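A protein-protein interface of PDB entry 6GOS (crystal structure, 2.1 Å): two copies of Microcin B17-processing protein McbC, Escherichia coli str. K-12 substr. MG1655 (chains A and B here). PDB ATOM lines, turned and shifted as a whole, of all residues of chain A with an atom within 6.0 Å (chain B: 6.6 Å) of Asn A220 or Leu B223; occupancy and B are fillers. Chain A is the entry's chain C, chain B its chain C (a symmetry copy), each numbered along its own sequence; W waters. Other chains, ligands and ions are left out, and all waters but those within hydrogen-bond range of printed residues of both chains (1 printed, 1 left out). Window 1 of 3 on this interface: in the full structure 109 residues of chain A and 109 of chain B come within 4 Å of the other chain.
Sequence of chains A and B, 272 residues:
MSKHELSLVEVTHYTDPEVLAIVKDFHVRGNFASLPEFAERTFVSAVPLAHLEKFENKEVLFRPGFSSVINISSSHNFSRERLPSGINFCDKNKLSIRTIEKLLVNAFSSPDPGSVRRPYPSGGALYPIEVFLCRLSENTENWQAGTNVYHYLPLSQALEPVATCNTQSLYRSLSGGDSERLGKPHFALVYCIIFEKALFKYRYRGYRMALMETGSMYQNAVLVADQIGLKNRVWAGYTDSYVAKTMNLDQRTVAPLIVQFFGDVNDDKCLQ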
ATOM      1  N   LEU A 103     -18.543  19.110  15.767  1.00  0.00           N
ATOM      2  CA  LEU A 103     -17.736  18.207  16.573  1.00  0.00           C
ATOM      3  C   LEU A 103     -16.721  17.442  15.702  1.00  0.00           C
ATOM      4  O   LEU A 103     -15.519  17.440  15.986  1.00  0.00           O
ATOM      5  CB  LEU A 103     -18.625  17.225  17.356  1.00  0.00           C
ATOM      6  CG  LEU A 103     -17.908  16.125  18.157  1.00  0.00           C
ATOM      7  CD1 LEU A 103     -16.962  16.723  19.185  1.00  0.00           C
ATOM      8  CD2 LEU A 103     -18.917  15.222  18.844  1.00  0.00           C
ATOM      9  N   ASN A 106     -13.740  19.475  13.825  1.00  0.00           N
ATOM     10  CA  ASN A 106     -12.804  20.057  14.786  1.00  0.00           C
ATOM     11  C   ASN A 106     -12.009  18.983  15.526  1.00  0.00           C
ATOM     12  O   ASN A 106     -10.807  19.140  15.741  1.00  0.00           O
ATOM     13  CB  ASN A 106     -13.541  20.950  15.786  1.00  0.00           C
ATOM     14  CG  ASN A 106     -13.955  22.281  15.180  1.00  0.00           C
ATOM     15  OD1 ASN A 106     -13.111  23.181  14.981  1.00  0.00           O
ATOM     16  ND2 ASN A 106     -15.249  22.418  14.865  1.00  0.00           N
ATOM     17  N   ALA A 107     -12.677  17.899  15.918  1.00  0.00           N
ATOM     18  CA  ALA A 107     -11.996  16.805  16.617  1.00  0.00           C
ATOM     19  C   ALA A 107     -10.988  16.035  15.750  1.00  0.00           C
ATOM     20  O   ALA A 107      -9.938  15.608  16.242  1.00  0.00           O
ATOM     21  CB  ALA A 107     -13.018  15.835  17.182  1.00  0.00           C
ATOM     22  N   PHE A 108     -11.319  15.820  14.480  1.00  0.00           N
ATOM     23  CA  PHE A 108     -10.618  14.790  13.681  1.00  0.00           C
ATOM     24  C   PHE A 108     -10.033  15.250  12.342  1.00  0.00           C
ATOM     25  O   PHE A 108      -9.367  14.445  11.656  1.00  0.00           O
ATOM     26  CB  PHE A 108     -11.572  13.623  13.406  1.00  0.00           C
ATOM     27  CG  PHE A 108     -12.299  13.115  14.628  1.00  0.00           C
ATOM     28  CD1 PHE A 108     -11.597  12.743  15.776  1.00  0.00           C
ATOM     29  CD2 PHE A 108     -13.688  12.988  14.627  1.00  0.00           C
ATOM     30  CE1 PHE A 108     -12.265  12.272  16.894  1.00  0.00           C
ATOM     31  CE2 PHE A 108     -14.350  12.505  15.741  1.00  0.00           C
ATOM     32  CZ  PHE A 108     -13.642  12.145  16.873  1.00  0.00           C
ATOM     33  N   PRO A 119      -5.577  16.657  13.430  1.00  0.00           N
ATOM     34  CA  PRO A 119      -5.247  17.269  14.722  1.00  0.00           C
ATOM     35  C   PRO A 119      -4.814  16.283  15.811  1.00  0.00           C
ATOM     36  O   PRO A 119      -4.789  16.643  16.978  1.00  0.00           O
ATOM     37  CB  PRO A 119      -6.545  18.001  15.113  1.00  0.00           C
ATOM     38  CG  PRO A 119      -7.619  17.272  14.403  1.00  0.00           C
ATOM     39  CD  PRO A 119      -7.013  16.768  13.124  1.00  0.00           C
ATOM     40  N   TYR A 120      -4.484  15.057  15.431  1.00  0.00           N
ATOM     41  CA  TYR A 120      -3.871  14.097  16.331  1.00  0.00           C
ATOM     42  C   TYR A 120      -2.853  13.333  15.519  1.00  0.00           C
ATOM     43  O   TYR A 120      -3.063  13.124  14.320  1.00  0.00           O
ATOM     44  CB  TYR A 120      -4.919  13.160  16.960  1.00  0.00           C
ATOM     45  CG  TYR A 120      -5.717  12.341  15.977  1.00  0.00           C
ATOM     46  CD1 TYR A 120      -6.817  12.885  15.301  1.00  0.00           C
ATOM     47  CD2 TYR A 120      -5.378  11.012  15.724  1.00  0.00           C
ATOM     48  CE1 TYR A 120      -7.546  12.130  14.390  1.00  0.00           C
ATOM     49  CE2 TYR A 120      -6.099  10.244  14.829  1.00  0.00           C
ATOM     50  CZ  TYR A 120      -7.179  10.800  14.158  1.00  0.00           C
ATOM     51  OH  TYR A 120      -7.866  10.007  13.267  1.00  0.00           O
ATOM     52  N   GLY A 215      -7.180   7.097  22.227  1.00  0.00           N
ATOM     53  CA  GLY A 215      -7.280   8.053  23.325  1.00  0.00           C
ATOM     54  C   GLY A 215      -6.987   9.481  22.923  1.00  0.00           C
ATOM     55  O   GLY A 215      -7.622  10.418  23.442  1.00  0.00           O
ATOM     56  N   SER A 216      -6.027   9.674  22.022  1.00  0.00           N
ATOM     57  CA  SER A 216      -5.796  11.001  21.460  1.00  0.00           C
ATOM     58  C   SER A 216      -7.055  11.499  20.772  1.00  0.00           C
ATOM     59  O   SER A 216      -7.387  12.676  20.886  1.00  0.00           O
ATOM     60  CB  SER A 216      -4.590  11.029  20.498  1.00  0.00           C
ATOM     61  OG  SER A 216      -4.845  10.334  19.310  1.00  0.00           O
ATOM     62  N   MET A 217      -7.774  10.599  20.100  1.00  0.00           N
ATOM     63  CA  MET A 217      -8.977  10.983  19.347  1.00  0.00           C
ATOM     64  C   MET A 217     -10.152  11.351  20.231  1.00  0.00           C
ATOM     65  O   MET A 217     -10.717  12.446  20.079  1.00  0.00           O
ATOM     66  CB  MET A 217      -9.381   9.891  18.373  1.00  0.00           C
ATOM     67  CG  MET A 217      -8.351   9.731  17.280  1.00  0.00           C
ATOM     68  SD  MET A 217      -8.595   8.222  16.365  1.00  0.00           S
ATOM     69  CE  MET A 217     -10.092   8.528  15.456  1.00  0.00           C
ATOM     70  N   TYR A 218     -10.525  10.479  21.170  1.00  0.00           N
ATOM     71  CA  TYR A 218     -11.623  10.847  22.057  1.00  0.00           C
ATOM     72  C   TYR A 218     -11.320  12.076  22.895  1.00  0.00           C
ATOM     73  O   TYR A 218     -12.256  12.800  23.267  1.00  0.00           O
ATOM     74  CB  TYR A 218     -12.184   9.685  22.905  1.00  0.00           C
ATOM     75  CG  TYR A 218     -11.374   9.078  24.040  1.00  0.00           C
ATOM     76  CD1 TYR A 218     -10.987   9.824  25.150  1.00  0.00           C
ATOM     77  CD2 TYR A 218     -11.100   7.705  24.061  1.00  0.00           C
ATOM     78  CE1 TYR A 218     -10.290   9.236  26.202  1.00  0.00           C
ATOM     79  CE2 TYR A 218     -10.409   7.117  25.116  1.00  0.00           C
ATOM     80  CZ  TYR A 218     -10.012   7.892  26.190  1.00  0.00           C
ATOM     81  OH  TYR A 218      -9.316   7.324  27.236  1.00  0.00           O
ATOM     82  N   GLN A 219     -10.036  12.328  23.170  1.00  0.00           N
ATOM     83  CA  GLN A 219      -9.646  13.498  23.947  1.00  0.00           C
ATOM     84  C   GLN A 219      -9.934  14.780  23.198  1.00  0.00           C
ATOM     85  O   GLN A 219     -10.501  15.694  23.769  1.00  0.00           O
ATOM     86  CB  GLN A 219      -8.171  13.455  24.349  1.00  0.00           C
ATOM     87  CG  GLN A 219      -7.710  14.564  25.282  1.00  0.00           C
ATOM     88  CD  GLN A 219      -8.443  14.623  26.631  1.00  0.00           C
ATOM     89  OE1 GLN A 219      -9.059  13.644  27.081  1.00  0.00           O
ATOM     90  NE2 GLN A 219      -8.356  15.782  27.284  1.00  0.00           N
ATOM     91  N   ASN A 220      -9.517  14.856  21.940  1.00  0.00           N
ATOM     92  CA  ASN A 220      -9.929  15.955  21.063  1.00  0.00           C
ATOM     93  C   ASN A 220     -11.463  16.112  21.076  1.00  0.00           C
ATOM     94  O   ASN A 220     -11.963  17.238  21.112  1.00  0.00           O
ATOM     95  CB  ASN A 220      -9.499  15.714  19.613  1.00  0.00           C
ATOM     96  CG  ASN A 220      -8.077  16.137  19.322  1.00  0.00           C
ATOM     97  OD1 ASN A 220      -7.329  16.514  20.219  1.00  0.00           O
ATOM     98  ND2 ASN A 220      -7.694  16.065  18.037  1.00  0.00           N
ATOM     99  N   ALA A 221     -12.202  15.000  21.028  1.00  0.00           N
ATOM    100  CA  ALA A 221     -13.670  15.081  21.076  1.00  0.00           C
ATOM    101  C   ALA A 221     -14.198  15.650  22.396  1.00  0.00           C
ATOM    102  O   ALA A 221     -15.138  16.443  22.376  1.00  0.00           O
ATOM    103  CB  ALA A 221     -14.326  13.752  20.771  1.00  0.00           C
ATOM    104  N   VAL A 222     -13.584  15.252  23.514  1.00  0.00           N
ATOM    105  CA  VAL A 222     -13.883  15.813  24.840  1.00  0.00           C
ATOM    106  C   VAL A 222     -13.716  17.318  24.863  1.00  0.00           C
ATOM    107  O   VAL A 222     -14.585  18.049  25.343  1.00  0.00           O
ATOM    108  CB  VAL A 222     -12.988  15.193  25.961  1.00  0.00           C
ATOM    109  CG1 VAL A 222     -13.085  15.959  27.276  1.00  0.00           C
ATOM    110  CG2 VAL A 222     -13.386  13.749  26.206  1.00  0.00           C
ATOM    111  N   LEU A 223     -12.574  17.768  24.375  1.00  0.00           N
ATOM    112  CA  LEU A 223     -12.233  19.181  24.437  1.00  0.00           C
ATOM    113  C   LEU A 223     -13.131  19.986  23.511  1.00  0.00           C
ATOM    114  O   LEU A 223     -13.609  21.041  23.895  1.00  0.00           O
ATOM    115  CB  LEU A 223     -10.760  19.381  24.087  1.00  0.00           C
ATOM    116  CG  LEU A 223      -9.787  18.735  25.085  1.00  0.00           C
ATOM    117  CD1 LEU A 223      -8.359  18.823  24.554  1.00  0.00           C
ATOM    118  CD2 LEU A 223      -9.916  19.366  26.475  1.00  0.00           C
ATOM    119  N   VAL A 224     -13.382  19.466  22.312  1.00  0.00           N
ATOM    120  CA  VAL A 224     -14.242  20.149  21.352  1.00  0.00           C
ATOM    121  C   VAL A 224     -15.676  20.205  21.886  1.00  0.00           C
ATOM    122  O   VAL A 224     -16.331  21.260  21.814  1.00  0.00           O
ATOM    123  CB  VAL A 224     -14.208  19.475  19.966  1.00  0.00           C
ATOM    124  CG1 VAL A 224     -15.276  20.066  19.043  1.00  0.00           C
ATOM    125  CG2 VAL A 224     -12.827  19.622  19.334  1.00  0.00           C
ATOM    126  N   ALA A 225     -16.142  19.070  22.404  1.00  0.00           N
ATOM    127  CA  ALA A 225     -17.474  18.950  23.016  1.00  0.00           C
ATOM    128  C   ALA A 225     -17.740  19.993  24.087  1.00  0.00           C
ATOM    129  O   ALA A 225     -18.814  20.601  24.107  1.00  0.00           O
ATOM    130  CB  ALA A 225     -17.659  17.557  23.597  1.00  0.00           C
ATOM    131  N   ARG B  82      -2.814  21.533  13.783  1.00  0.00           N
ATOM    132  CA  ARG B  82      -1.781  20.988  14.656  1.00  0.00           C
ATOM    133  C   ARG B  82      -0.462  21.213  13.950  1.00  0.00           C
ATOM    134  O   ARG B  82      -0.398  21.097  12.721  1.00  0.00           O
ATOM    135  CB  ARG B  82      -2.008  19.503  14.924  1.00  0.00           C
ATOM    136  CG  ARG B  82      -0.951  18.847  15.803  1.00  0.00           C
ATOM    137  CD  ARG B  82      -1.265  17.390  16.114  1.00  0.00           C
ATOM    138  NE  ARG B  82      -1.522  16.623  14.900  1.00  0.00           N
ATOM    139  CZ  ARG B  82      -0.618  15.951  14.191  1.00  0.00           C
ATOM    140  NH1 ARG B  82       0.660  15.926  14.552  1.00  0.00           N
ATOM    141  NH2 ARG B  82      -1.007  15.293  13.096  1.00  0.00           N
ATOM    142  N   TYR B 218      -0.991  12.297  26.246  1.00  0.00           N
ATOM    143  CA  TYR B 218      -0.055  12.912  25.311  1.00  0.00           C
ATOM    144  C   TYR B 218      -0.723  13.894  24.365  1.00  0.00           C
ATOM    145  O   TYR B 218      -0.062  14.841  23.912  1.00  0.00           O
ATOM    146  CB  TYR B 218       0.861  11.916  24.568  1.00  0.00           C
ATOM    147  CG  TYR B 218       0.307  10.978  23.507  1.00  0.00           C
ATOM    148  CD1 TYR B 218      -0.282  11.452  22.338  1.00  0.00           C
ATOM    149  CD2 TYR B 218       0.487   9.593  23.620  1.00  0.00           C
ATOM    150  CE1 TYR B 218      -0.738  10.575  21.358  1.00  0.00           C
ATOM    151  CE2 TYR B 218       0.037   8.719  22.636  1.00  0.00           C
ATOM    152  CZ  TYR B 218      -0.571   9.221  21.500  1.00  0.00           C
ATOM    153  OH  TYR B 218      -1.032   8.364  20.523  1.00  0.00           O
ATOM    154  N   GLN B 219      -2.016  13.694  24.088  1.00  0.00           N
ATOM    155  CA  GLN B 219      -2.747  14.600  23.210  1.00  0.00           C
ATOM    156  C   GLN B 219      -2.897  15.971  23.830  1.00  0.00           C
ATOM    157  O   GLN B 219      -2.643  16.960  23.167  1.00  0.00           O
ATOM    158  CB  GLN B 219      -4.124  14.048  22.837  1.00  0.00           C
ATOM    159  CG  GLN B 219      -4.902  14.858  21.811  1.00  0.00           C
ATOM    160  CD  GLN B 219      -4.206  15.022  20.452  1.00  0.00           C
ATOM    161  OE1 GLN B 219      -3.301  14.253  20.086  1.00  0.00           O
ATOM    162  NE2 GLN B 219      -4.648  16.025  19.693  1.00  0.00           N
ATOM    163  N   ASN B 220      -3.335  16.027  25.082  1.00  0.00           N
ATOM    164  CA  ASN B 220      -3.310  17.278  25.845  1.00  0.00           C
ATOM    165  C   ASN B 220      -1.907  17.916  25.793  1.00  0.00           C
ATOM    166  O   ASN B 220      -1.794  19.134  25.644  1.00  0.00           O
ATOM    167  CB  ASN B 220      -3.663  17.050  27.318  1.00  0.00           C
ATOM    168  CG  ASN B 220      -5.150  17.021  27.589  1.00  0.00           C
ATOM    169  OD1 ASN B 220      -5.966  17.052  26.673  1.00  0.00           O
ATOM    170  ND2 ASN B 220      -5.510  16.951  28.882  1.00  0.00           N
ATOM    171  N   ALA B 221      -0.852  17.109  25.934  1.00  0.00           N
ATOM    172  CA  ALA B 221       0.513  17.651  25.856  1.00  0.00           C
ATOM    173  C   ALA B 221       0.852  18.232  24.480  1.00  0.00           C
ATOM    174  O   ALA B 221       1.487  19.282  24.411  1.00  0.00           O
ATOM    175  CB  ALA B 221       1.555  16.637  26.275  1.00  0.00           C
ATOM    176  N   VAL B 222       0.415  17.555  23.415  1.00  0.00           N
ATOM    177  CA  VAL B 222       0.539  18.054  22.037  1.00  0.00           C
ATOM    178  C   VAL B 222      -0.101  19.417  21.875  1.00  0.00           C
ATOM    179  O   VAL B 222       0.496  20.340  21.314  1.00  0.00           O
ATOM    180  CB  VAL B 222      -0.093  17.078  20.994  1.00  0.00           C
ATOM    181  CG1 VAL B 222      -0.226  17.706  19.611  1.00  0.00           C
ATOM    182  CG2 VAL B 222       0.750  15.821  20.880  1.00  0.00           C
ATOM    183  N   LEU B 223      -1.334  19.522  22.336  1.00  0.00           N
ATOM    184  CA  LEU B 223      -2.108  20.738  22.146  1.00  0.00           C
ATOM    185  C   LEU B 223      -1.531  21.872  22.978  1.00  0.00           C
ATOM    186  O   LEU B 223      -1.409  22.984  22.490  1.00  0.00           O
ATOM    187  CB  LEU B 223      -3.573  20.489  22.499  1.00  0.00           C
ATOM    188  CG  LEU B 223      -4.273  19.473  21.581  1.00  0.00           C
ATOM    189  CD1 LEU B 223      -5.662  19.150  22.124  1.00  0.00           C
ATOM    190  CD2 LEU B 223      -4.331  19.979  20.136  1.00  0.00           C
ATOM    191  N   VAL B 224      -1.145  21.576  24.217  1.00  0.00           N
ATOM    192  CA  VAL B 224      -0.563  22.585  25.095  1.00  0.00           C
ATOM    193  C   VAL B 224       0.785  23.047  24.536  1.00  0.00           C
ATOM    194  O   VAL B 224       1.066  24.258  24.498  1.00  0.00           O
ATOM    195  CB  VAL B 224      -0.402  22.070  26.539  1.00  0.00           C
ATOM    196  CG1 VAL B 224       0.407  23.056  27.385  1.00  0.00           C
ATOM    197  CG2 VAL B 224      -1.767  21.826  27.175  1.00  0.00           C
ATOM    198  N   ALA B 225       1.598  22.077  24.120  1.00  0.00           N
ATOM    199  CA  ALA B 225       2.908  22.333  23.501  1.00  0.00           C
ATOM    200  C   ALA B 225       2.842  23.300  22.332  1.00  0.00           C
ATOM    201  O   ALA B 225       3.665  24.216  22.239  1.00  0.00           O
ATOM    202  CB  ALA B 225       3.538  21.024  23.052  1.00  0.00           C
ATOM    203  N   ASP B 226       1.858  23.100  21.459  1.00  0.00           N
ATOM    204  CA  ASP B 226       1.639  23.999  20.321  1.00  0.00           C
ATOM    205  C   ASP B 226       1.323  25.433  20.767  1.00  0.00           C
ATOM    206  O   ASP B 226       1.807  26.383  20.163  1.00  0.00           O
ATOM    207  CB  ASP B 226       0.512  23.475  19.414  1.00  0.00           C
ATOM    208  CG  ASP B 226       0.956  22.343  18.494  1.00  0.00           C
ATOM    209  OD1 ASP B 226       1.753  21.474  18.891  1.00  0.00           O
ATOM    210  OD2 ASP B 226       0.481  22.311  17.354  1.00  0.00           O
ATOM    211  N   GLN B 227       0.519  25.591  21.818  1.00  0.00           N
ATOM    212  CA  GLN B 227       0.132  26.930  22.302  1.00  0.00           C
ATOM    213  C   GLN B 227       1.227  27.680  23.023  1.00  0.00           C
ATOM    214  O   GLN B 227       1.154  28.886  23.113  1.00  0.00           O
ATOM    215  CB  GLN B 227      -1.029  26.854  23.284  1.00  0.00           C
ATOM    216  CG  GLN B 227      -2.328  26.320  22.736  1.00  0.00           C
ATOM    217  CD  GLN B 227      -3.296  26.060  23.864  1.00  0.00           C
ATOM    218  OE1 GLN B 227      -3.816  26.998  24.465  1.00  0.00           O
ATOM    219  NE2 GLN B 227      -3.528  24.799  24.172  1.00  0.00           N
ATOM    220  N   ILE B 228       2.197  26.979  23.596  1.00  0.00           N
ATOM    221  CA  ILE B 228       3.268  27.652  24.343  1.00  0.00           C
ATOM    222  C   ILE B 228       4.574  27.755  23.564  1.00  0.00           C
ATOM    223  O   ILE B 228       5.573  28.186  24.121  1.00  0.00           O
ATOM    224  CB  ILE B 228       3.509  27.001  25.732  1.00  0.00           C
ATOM    225  CG1 ILE B 228       4.069  25.577  25.610  1.00  0.00           C
ATOM    226  CG2 ILE B 228       2.225  27.023  26.564  1.00  0.00           C
ATOM    227  CD1 ILE B 228       4.253  24.909  26.950  1.00  0.00           C
ATOM    228  N   ASN B 232       6.993  19.196  19.421  1.00  0.00           N
ATOM    229  CA  ASN B 232       7.008  17.876  20.055  1.00  0.00           C
ATOM    230  C   ASN B 232       6.891  16.730  19.058  1.00  0.00           C
ATOM    231  O   ASN B 232       6.453  16.918  17.923  1.00  0.00           O
ATOM    232  CB  ASN B 232       5.867  17.756  21.057  1.00  0.00           C
ATOM    233  CG  ASN B 232       4.557  17.370  20.394  1.00  0.00           C
ATOM    234  OD1 ASN B 232       4.156  16.199  20.410  1.00  0.00           O
ATOM    235  ND2 ASN B 232       3.918  18.335  19.751  1.00  0.00           N
ATOM    236  N   GLN B 260       7.588  11.021  24.625  1.00  0.00           N
ATOM    237  CA  GLN B 260       7.205  12.201  23.857  1.00  0.00           C
ATOM    238  C   GLN B 260       8.302  13.232  24.040  1.00  0.00           C
ATOM    239  O   GLN B 260       8.570  13.651  25.181  1.00  0.00           O
ATOM    240  CB  GLN B 260       5.873  12.746  24.328  1.00  0.00           C
ATOM    241  CG  GLN B 260       5.376  13.937  23.524  1.00  0.00           C
ATOM    242  CD  GLN B 260       3.976  14.347  23.891  1.00  0.00           C
ATOM    243  OE1 GLN B 260       3.447  13.971  24.946  1.00  0.00           O
ATOM    244  NE2 GLN B 260       3.348  15.115  23.010  1.00  0.00           N
HETATM  245  O   HOH W   1      -2.395   9.691  18.672  1.00  0.00           O
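O of Pro A119 lies within hydrogen-bond range of NE2 of Gln B219. NH2 of Arg B82 is in hydrogen-bond range of O of Tyr A120 (3.2 Å). The side-chain amide nitrogen (NE2) of Gln A219 is in hydrogen-bond range of the side-chain amide oxygen (OD1) of Asn B220. The side-chain amide oxygen (OD1) of Asn A220 is in hydrogen-bond range of the side-chain amide nitrogen (NE2) of Gln B219, 2.8 Å away.
The backbone carbonyl oxygen (O) of Ala A107 is in hydrogen-bond range of the side-chain amide nitrogen (ND2) of Asn A220. The side-chain amide nitrogen (ND2) of Asn A220 lies within hydrogen-bond range of the backbone carbonyl oxygen (O) of Pro A119 (3.1 Å). The side-chain hydroxyl (OH) of Tyr A120 lies close to the side-chain sulfur (SD) of Met A217 (3.6 Å). The side-chain amide nitrogen (NE2) of Gln B227 is in hydrogen-bond range of the backbone carbonyl oxygen (O) of Leu B223 (3.3 Å).
Among the printed residues, merely in contact across the chains: Pro A119 with Arg B82 (3.4 Å), Ser A216 with Gln B219 (3.4 Å), Leu A223 with Leu B223 (3.6 Å), Leu A223 with Asn B220 (3.7 Å), Asn A220 with Leu B223 (3.7 Å), Tyr A120 with Gln B219 (3.7 Å) and Ser A216 with Tyr B218 (3.97 Å).
Of the printed residues of chain B, Pro A119 touches Arg B82 (3.4 Å) and Gln B219 (2.8 Å). Of the printed residues of chain B, Tyr A120 touches Arg B82 and Gln B219. Of the printed residues of chain B, Gln A219 touches Asn B220. Asn A220 touches just these residues of chain B: Gln B219 (2.8 Å) and Leu B223 (3.7 Å). Of the printed residues of chain A, Tyr B218 touches Ser A216. Printed residues of chain A within 4 Å of Gln B219: Pro A119, Tyr A120, Ser A216 and Asn A220. Ala B225 touches none of the printed residues of chain A. The nearest residue of chain A that does not touch Leu B223 is Pro A119 (4.6 Å).
Printed residues of chain B that touch a printed residue of chain A: Arg B82, Tyr B218, Gln B219, Asn B220 and Leu B223. Hydrophobic or aromatic side chains of chain B within 4 Å of the printed part of chain A: Tyr B218 and Leu B223. Of the 17 printed residues of chain A, 6 touch a printed residue of chain B. Among the printed residues, 11 pairs touch across the chains. Among the printed residues, no Asp or Glu carboxylate lies within 4 Å of a Lys or Arg side-chain nitrogen of the other chain.
Gln A219 touches Asn B220, and with the chains exchanged Asn A220 touches Gln B219. Asn A220 touches Leu B223, and with the chains exchanged Leu A223 touches Asn B220. Leu A223 touches its own counterpart, Leu B223. Positions printed for both chains: 218, 219, 220, 221, 222, 223, 224 and 225. Of the 11 pairs that touch across the chains among the printed residues, 5 have their exchanged pair printed and touching as well.
Water W1 lies within hydrogen-bond range of OG of Ser A216 (2.6 Å) and OH of Tyr B218 (2.7 Å).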
